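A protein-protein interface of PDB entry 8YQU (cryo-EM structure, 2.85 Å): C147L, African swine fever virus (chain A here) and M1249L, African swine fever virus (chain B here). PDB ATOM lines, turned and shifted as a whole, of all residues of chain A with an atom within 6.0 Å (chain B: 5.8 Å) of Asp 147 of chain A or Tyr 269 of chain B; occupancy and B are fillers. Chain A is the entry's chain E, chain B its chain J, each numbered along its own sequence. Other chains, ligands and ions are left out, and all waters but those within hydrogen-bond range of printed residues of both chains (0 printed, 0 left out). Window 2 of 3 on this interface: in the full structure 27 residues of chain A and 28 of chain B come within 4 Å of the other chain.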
ATOM      1  N   LYS A 107       6.624 -37.463  27.689  1.00  0.00           N
ATOM      2  CA  LYS A 107       5.477 -36.563  27.756  1.00  0.00           C
ATOM      3  C   LYS A 107       5.652 -35.371  26.828  1.00  0.00           C
ATOM      4  O   LYS A 107       4.719 -34.993  26.111  1.00  0.00           O
ATOM      5  CB  LYS A 107       5.255 -36.089  29.192  1.00  0.00           C
ATOM      6  CG  LYS A 107       4.759 -37.160  30.139  1.00  0.00           C
ATOM      7  CD  LYS A 107       4.635 -36.612  31.549  1.00  0.00           C
ATOM      8  CE  LYS A 107       3.496 -35.613  31.643  1.00  0.00           C
ATOM      9  NZ  LYS A 107       2.171 -36.259  31.452  1.00  0.00           N
ATOM     10  N   GLN A 108       6.841 -34.764  26.823  1.00  0.00           N
ATOM     11  CA  GLN A 108       7.062 -33.615  25.952  1.00  0.00           C
ATOM     12  C   GLN A 108       7.065 -34.017  24.482  1.00  0.00           C
ATOM     13  O   GLN A 108       6.631 -33.236  23.630  1.00  0.00           O
ATOM     14  CB  GLN A 108       8.367 -32.912  26.319  1.00  0.00           C
ATOM     15  CG  GLN A 108       8.433 -32.461  27.764  1.00  0.00           C
ATOM     16  CD  GLN A 108       7.364 -31.446  28.107  1.00  0.00           C
ATOM     17  OE1 GLN A 108       7.155 -30.478  27.378  1.00  0.00           O
ATOM     18  NE2 GLN A 108       6.675 -31.665  29.220  1.00  0.00           N
ATOM     19  N   PHE A 111       3.485 -34.260  23.597  1.00  0.00           N
ATOM     20  CA  PHE A 111       2.864 -32.941  23.561  1.00  0.00           C
ATOM     21  C   PHE A 111       3.363 -32.120  22.378  1.00  0.00           C
ATOM     22  O   PHE A 111       2.601 -31.344  21.790  1.00  0.00           O
ATOM     23  CB  PHE A 111       3.128 -32.210  24.874  1.00  0.00           C
ATOM     24  CG  PHE A 111       2.478 -32.853  26.063  1.00  0.00           C
ATOM     25  CD1 PHE A 111       1.341 -33.628  25.912  1.00  0.00           C
ATOM     26  CD2 PHE A 111       2.999 -32.677  27.332  1.00  0.00           C
ATOM     27  CE1 PHE A 111       0.738 -34.216  27.004  1.00  0.00           C
ATOM     28  CE2 PHE A 111       2.401 -33.267  28.426  1.00  0.00           C
ATOM     29  CZ  PHE A 111       1.270 -34.036  28.263  1.00  0.00           C
ATOM     30  N   ASN A 112       4.634 -32.272  22.019  1.00  0.00           N
ATOM     31  CA  ASN A 112       5.214 -31.564  20.888  1.00  0.00           C
ATOM     32  C   ASN A 112       4.987 -32.283  19.567  1.00  0.00           C
ATOM     33  O   ASN A 112       5.483 -31.819  18.535  1.00  0.00           O
ATOM     34  CB  ASN A 112       6.715 -31.353  21.107  1.00  0.00           C
ATOM     35  CG  ASN A 112       7.007 -30.268  22.123  1.00  0.00           C
ATOM     36  OD1 ASN A 112       6.705 -29.097  21.901  1.00  0.00           O
ATOM     37  ND2 ASN A 112       7.591 -30.656  23.251  1.00  0.00           N
ATOM     38  N   LEU A 145      -4.151 -35.534  27.900  1.00  0.00           N
ATOM     39  CA  LEU A 145      -3.402 -35.325  29.129  1.00  0.00           C
ATOM     40  C   LEU A 145      -3.283 -33.833  29.436  1.00  0.00           C
ATOM     41  O   LEU A 145      -3.688 -32.970  28.651  1.00  0.00           O
ATOM     42  CB  LEU A 145      -2.027 -35.979  29.030  1.00  0.00           C
ATOM     43  CG  LEU A 145      -2.010 -37.461  28.650  1.00  0.00           C
ATOM     44  CD1 LEU A 145      -0.586 -37.940  28.426  1.00  0.00           C
ATOM     45  CD2 LEU A 145      -2.700 -38.299  29.715  1.00  0.00           C
ATOM     46  N   LEU A 146      -2.715 -33.526  30.599  1.00  0.00           N
ATOM     47  CA  LEU A 146      -2.568 -32.152  31.054  1.00  0.00           C
ATOM     48  C   LEU A 146      -1.169 -31.944  31.611  1.00  0.00           C
ATOM     49  O   LEU A 146      -0.623 -32.821  32.287  1.00  0.00           O
ATOM     50  CB  LEU A 146      -3.640 -31.800  32.102  1.00  0.00           C
ATOM     51  CG  LEU A 146      -3.735 -32.574  33.426  1.00  0.00           C
ATOM     52  CD1 LEU A 146      -2.780 -32.048  34.495  1.00  0.00           C
ATOM     53  CD2 LEU A 146      -5.167 -32.566  33.940  1.00  0.00           C
ATOM     54  N   ASP A 147      -0.593 -30.781  31.314  1.00  0.00           N
ATOM     55  CA  ASP A 147       0.726 -30.404  31.816  1.00  0.00           C
ATOM     56  C   ASP A 147       0.991 -28.926  31.547  1.00  0.00           C
ATOM     57  O   ASP A 147       1.838 -28.310  32.193  1.00  0.00           O
ATOM     58  CB  ASP A 147       1.822 -31.258  31.177  1.00  0.00           C
ATOM     59  CG  ASP A 147       3.124 -31.213  31.953  1.00  0.00           C
ATOM     60  OD1 ASP A 147       3.898 -30.253  31.763  1.00  0.00           O
ATOM     61  OD2 ASP A 147       3.372 -32.139  32.754  1.00  0.00           O
ATOM     62  N   LEU B 265       3.379 -19.528  19.787  1.00  0.00           N
ATOM     63  CA  LEU B 265       3.572 -20.170  21.083  1.00  0.00           C
ATOM     64  C   LEU B 265       4.389 -21.455  20.995  1.00  0.00           C
ATOM     65  O   LEU B 265       4.916 -21.909  22.017  1.00  0.00           O
ATOM     66  CB  LEU B 265       2.207 -20.463  21.713  1.00  0.00           C
ATOM     67  CG  LEU B 265       2.136 -21.071  23.114  1.00  0.00           C
ATOM     68  CD1 LEU B 265       2.741 -20.126  24.135  1.00  0.00           C
ATOM     69  CD2 LEU B 265       0.701 -21.415  23.478  1.00  0.00           C
ATOM     70  N   SER B 266       4.510 -22.044  19.802  1.00  0.00           N
ATOM     71  CA  SER B 266       5.202 -23.323  19.666  1.00  0.00           C
ATOM     72  C   SER B 266       6.653 -23.228  20.121  1.00  0.00           C
ATOM     73  O   SER B 266       7.153 -24.123  20.814  1.00  0.00           O
ATOM     74  CB  SER B 266       5.125 -23.806  18.217  1.00  0.00           C
ATOM     75  OG  SER B 266       5.839 -22.940  17.353  1.00  0.00           O
ATOM     76  N   THR B 267       7.345 -22.152  19.745  1.00  0.00           N
ATOM     77  CA  THR B 267       8.714 -21.936  20.200  1.00  0.00           C
ATOM     78  C   THR B 267       8.789 -21.526  21.665  1.00  0.00           C
ATOM     79  O   THR B 267       9.876 -21.180  22.139  1.00  0.00           O
ATOM     80  CB  THR B 267       9.393 -20.870  19.339  1.00  0.00           C
ATOM     81  OG1 THR B 267       8.800 -19.593  19.604  1.00  0.00           O
ATOM     82  CG2 THR B 267       9.232 -21.200  17.863  1.00  0.00           C
ATOM     83  N   MET B 268       7.667 -21.557  22.383  1.00  0.00           N
ATOM     84  CA  MET B 268       7.578 -21.042  23.738  1.00  0.00           C
ATOM     85  C   MET B 268       6.924 -22.008  24.713  1.00  0.00           C
ATOM     86  O   MET B 268       7.116 -21.859  25.925  1.00  0.00           O
ATOM     87  CB  MET B 268       6.790 -19.724  23.737  1.00  0.00           C
ATOM     88  CG  MET B 268       7.487 -18.605  22.983  1.00  0.00           C
ATOM     89  SD  MET B 268       6.473 -17.126  22.839  1.00  0.00           S
ATOM     90  CE  MET B 268       6.467 -16.576  24.532  1.00  0.00           C
ATOM     91  N   TYR B 269       6.163 -22.984  24.223  1.00  0.00           N
ATOM     92  CA  TYR B 269       5.471 -23.955  25.055  1.00  0.00           C
ATOM     93  C   TYR B 269       5.394 -25.274  24.298  1.00  0.00           C
ATOM     94  O   TYR B 269       5.588 -25.324  23.082  1.00  0.00           O
ATOM     95  CB  TYR B 269       4.069 -23.460  25.439  1.00  0.00           C
ATOM     96  CG  TYR B 269       3.357 -24.314  26.463  1.00  0.00           C
ATOM     97  CD1 TYR B 269       3.945 -24.606  27.685  1.00  0.00           C
ATOM     98  CD2 TYR B 269       2.089 -24.817  26.210  1.00  0.00           C
ATOM     99  CE1 TYR B 269       3.293 -25.385  28.622  1.00  0.00           C
ATOM    100  CE2 TYR B 269       1.429 -25.594  27.141  1.00  0.00           C
ATOM    101  CZ  TYR B 269       2.035 -25.874  28.345  1.00  0.00           C
ATOM    102  OH  TYR B 269       1.379 -26.648  29.274  1.00  0.00           O
ATOM    103  N   SER B 270       5.113 -26.351  25.034  1.00  0.00           N
ATOM    104  CA  SER B 270       5.062 -27.694  24.457  1.00  0.00           C
ATOM    105  C   SER B 270       3.781 -27.853  23.637  1.00  0.00           C
ATOM    106  O   SER B 270       2.862 -28.601  23.976  1.00  0.00           O
ATOM    107  CB  SER B 270       5.156 -28.747  25.552  1.00  0.00           C
ATOM    108  OG  SER B 270       4.024 -28.697  26.404  1.00  0.00           O
ATOM    109  N   VAL B 271       3.735 -27.122  22.526  1.00  0.00           N
ATOM    110  CA  VAL B 271       2.595 -27.131  21.618  1.00  0.00           C
ATOM    111  C   VAL B 271       3.115 -27.147  20.187  1.00  0.00           C
ATOM    112  O   VAL B 271       4.034 -26.397  19.842  1.00  0.00           O
ATOM    113  CB  VAL B 271       1.673 -25.915  21.853  1.00  0.00           C
ATOM    114  CG1 VAL B 271       0.728 -25.719  20.678  1.00  0.00           C
ATOM    115  CG2 VAL B 271       0.885 -26.086  23.139  1.00  0.00           C
ATOM    116  N   SER B 272       2.529 -28.007  19.355  1.00  0.00           N
ATOM    117  CA  SER B 272       2.822 -28.036  17.931  1.00  0.00           C
ATOM    118  C   SER B 272       1.505 -27.937  17.171  1.00  0.00           C
ATOM    119  O   SER B 272       0.588 -28.741  17.414  1.00  0.00           O
ATOM    120  CB  SER B 272       3.579 -29.309  17.537  1.00  0.00           C
ATOM    121  OG  SER B 272       3.870 -29.318  16.151  1.00  0.00           O
ATOM    122  N   ASP B 285      -4.969 -28.532  22.877  1.00  0.00           N
ATOM    123  CA  ASP B 285      -3.750 -27.790  23.185  1.00  0.00           C
ATOM    124  C   ASP B 285      -4.064 -26.531  23.983  1.00  0.00           C
ATOM    125  O   ASP B 285      -3.388 -26.228  24.975  1.00  0.00           O
ATOM    126  CB  ASP B 285      -3.008 -27.443  21.896  1.00  0.00           C
ATOM    127  CG  ASP B 285      -2.337 -28.649  21.265  1.00  0.00           C
ATOM    128  OD1 ASP B 285      -1.998 -29.598  22.004  1.00  0.00           O
ATOM    129  OD2 ASP B 285      -2.149 -28.650  20.030  1.00  0.00           O
ATOM    130  N   ARG B 288      -5.143 -27.557  27.548  1.00  0.00           N
ATOM    131  CA  ARG B 288      -3.995 -27.994  28.333  1.00  0.00           C
ATOM    132  C   ARG B 288      -3.133 -26.810  28.747  1.00  0.00           C
ATOM    133  O   ARG B 288      -2.633 -26.761  29.876  1.00  0.00           O
ATOM    134  CB  ARG B 288      -3.188 -29.013  27.525  1.00  0.00           C
ATOM    135  CG  ARG B 288      -2.022 -29.680  28.241  1.00  0.00           C
ATOM    136  CD  ARG B 288      -0.747 -28.863  28.117  1.00  0.00           C
ATOM    137  NE  ARG B 288      -0.442 -28.572  26.721  1.00  0.00           N
ATOM    138  CZ  ARG B 288       0.151 -29.420  25.893  1.00  0.00           C
ATOM    139  NH1 ARG B 288       0.500 -30.632  26.283  1.00  0.00           N
ATOM    140  NH2 ARG B 288       0.389 -29.044  24.641  1.00  0.00           N
ATOM    141  N   ALA B 289      -2.949 -25.841  27.845  1.00  0.00           N
ATOM    142  CA  ALA B 289      -2.194 -24.644  28.191  1.00  0.00           C
ATOM    143  C   ALA B 289      -2.875 -23.812  29.267  1.00  0.00           C
ATOM    144  O   ALA B 289      -2.286 -22.830  29.731  1.00  0.00           O
ATOM    145  CB  ALA B 289      -1.964 -23.789  26.945  1.00  0.00           C
ATOM    146  N   ALA B 307       3.613 -17.183  29.100  1.00  0.00           N
ATOM    147  CA  ALA B 307       4.362 -18.370  28.703  1.00  0.00           C
ATOM    148  C   ALA B 307       5.856 -18.087  28.644  1.00  0.00           C
ATOM    149  O   ALA B 307       6.667 -18.916  29.076  1.00  0.00           O
ATOM    150  CB  ALA B 307       3.858 -18.881  27.355  1.00  0.00           C
ATOM    151  N   ARG B 310       7.035 -18.010  32.301  1.00  0.00           N
ATOM    152  CA  ARG B 310       7.070 -19.338  32.905  1.00  0.00           C
ATOM    153  C   ARG B 310       8.229 -20.164  32.361  1.00  0.00           C
ATOM    154  O   ARG B 310       8.917 -20.857  33.122  1.00  0.00           O
ATOM    155  CB  ARG B 310       5.736 -20.049  32.674  1.00  0.00           C
ATOM    156  CG  ARG B 310       5.801 -21.564  32.757  1.00  0.00           C
ATOM    157  CD  ARG B 310       4.458 -22.182  32.400  1.00  0.00           C
ATOM    158  NE  ARG B 310       4.182 -22.100  30.972  1.00  0.00           N
ATOM    159  CZ  ARG B 310       2.967 -22.002  30.448  1.00  0.00           C
ATOM    160  NH1 ARG B 310       1.887 -21.971  31.212  1.00  0.00           N
ATOM    161  NH2 ARG B 310       2.832 -21.930  29.128  1.00  0.00           N
ATOM    162  N   GLU B 311       8.473 -20.089  31.050  1.00  0.00           N
ATOM    163  CA  GLU B 311       9.643 -20.751  30.484  1.00  0.00           C
ATOM    164  C   GLU B 311      10.928 -20.195  31.085  1.00  0.00           C
ATOM    165  O   GLU B 311      11.890 -20.940  31.313  1.00  0.00           O
ATOM    166  CB  GLU B 311       9.647 -20.598  28.964  1.00  0.00           C
ATOM    167  CG  GLU B 311      10.721 -21.410  28.258  1.00  0.00           C
ATOM    168  CD  GLU B 311      10.977 -20.931  26.842  1.00  0.00           C
ATOM    169  OE1 GLU B 311      10.450 -19.862  26.470  1.00  0.00           O
ATOM    170  OE2 GLU B 311      11.705 -21.625  26.100  1.00  0.00           O
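Printed residues of chain B within 4 Å of Gln 108 of chain A: Ser 270.
Of the printed residues of chain B, Asn 112 of chain A touches Ser 270 (3.3 Å), Val 271 (3.6 Å) and Ser 272 (3.3 Å).
Of the printed residues of chain B, Leu 146 of chain A touches Arg 288 (3.8 Å).
Asp 147 of chain A touches just these residues of chain B: Tyr 269 (3.2 Å) and Arg 288 (3.6 Å).
Thr 267 of chain B touches none of the printed residues of chain A.
Of chain A, only Asp 147 (3.2 Å) comes within 4 Å of Tyr 269 of chain B.
The nearest residue of chain A that does not touch Tyr 269 of chain B is Asn 112 of chain A (4.1 Å).
The nearest printed residue of chain B that does not touch Gln 108 of chain A is Tyr 269 of chain B (6.3 Å).
Among the printed residues, pairs that only touch across the chains: Gln 108 of chain A with Ser 270 of chain B (3.2 Å), Phe 111 of chain A with Ser 270 of chain B (3.5 Å), Phe 111 of chain A with Arg 288 of chain B (3.0 Å), Asn 112 of chain A with Ser 270 of chain B (3.3 Å), Asn 112 of chain A with Val 271 of chain B (3.6 Å), Asn 112 of chain A with Ser 272 of chain B (3.3 Å), Leu 145 of chain A with Arg 288 of chain B (3.7 Å), Leu 146 of chain A with Arg 288 of chain B (3.8 Å) and Asp 147 of chain A with Arg 288 of chain B (3.6 Å).
Of the 14 printed residues of chain B, 5 touch a printed residue of chain A.
Of the 7 printed residues of chain A, 6 touch a printed residue of chain B.
Printed residues of chain A that touch a printed residue of chain B: Gln 108, Phe 111, Asn 112, Leu 145, Leu 146 and Asp 147.
Among the printed residues, no Asp or Glu carboxylate lies within 4 Å of a Lys or Arg side-chain nitrogen of the other chain.
The backbone carbonyl oxygen (O) of Asp 147 of chain A lies close to the side-chain hydroxyl (OH) of Tyr 269 of chain B (3.4 Å).
ND2 of Asn 112 of chain A lies within hydrogen-bond range of O of Gln 108 of chain A (2.8 Å).
The backbone carbonyl oxygen (O) of Ser 270 of chain B sits at hydrogen-bond distance from the guanidinium group (NH2) of Arg 288 of chain B.
OD1 of Asp 285 of chain B lies within salt-bridge range of NH2 of Arg 288 of chain B (3.6 Å).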
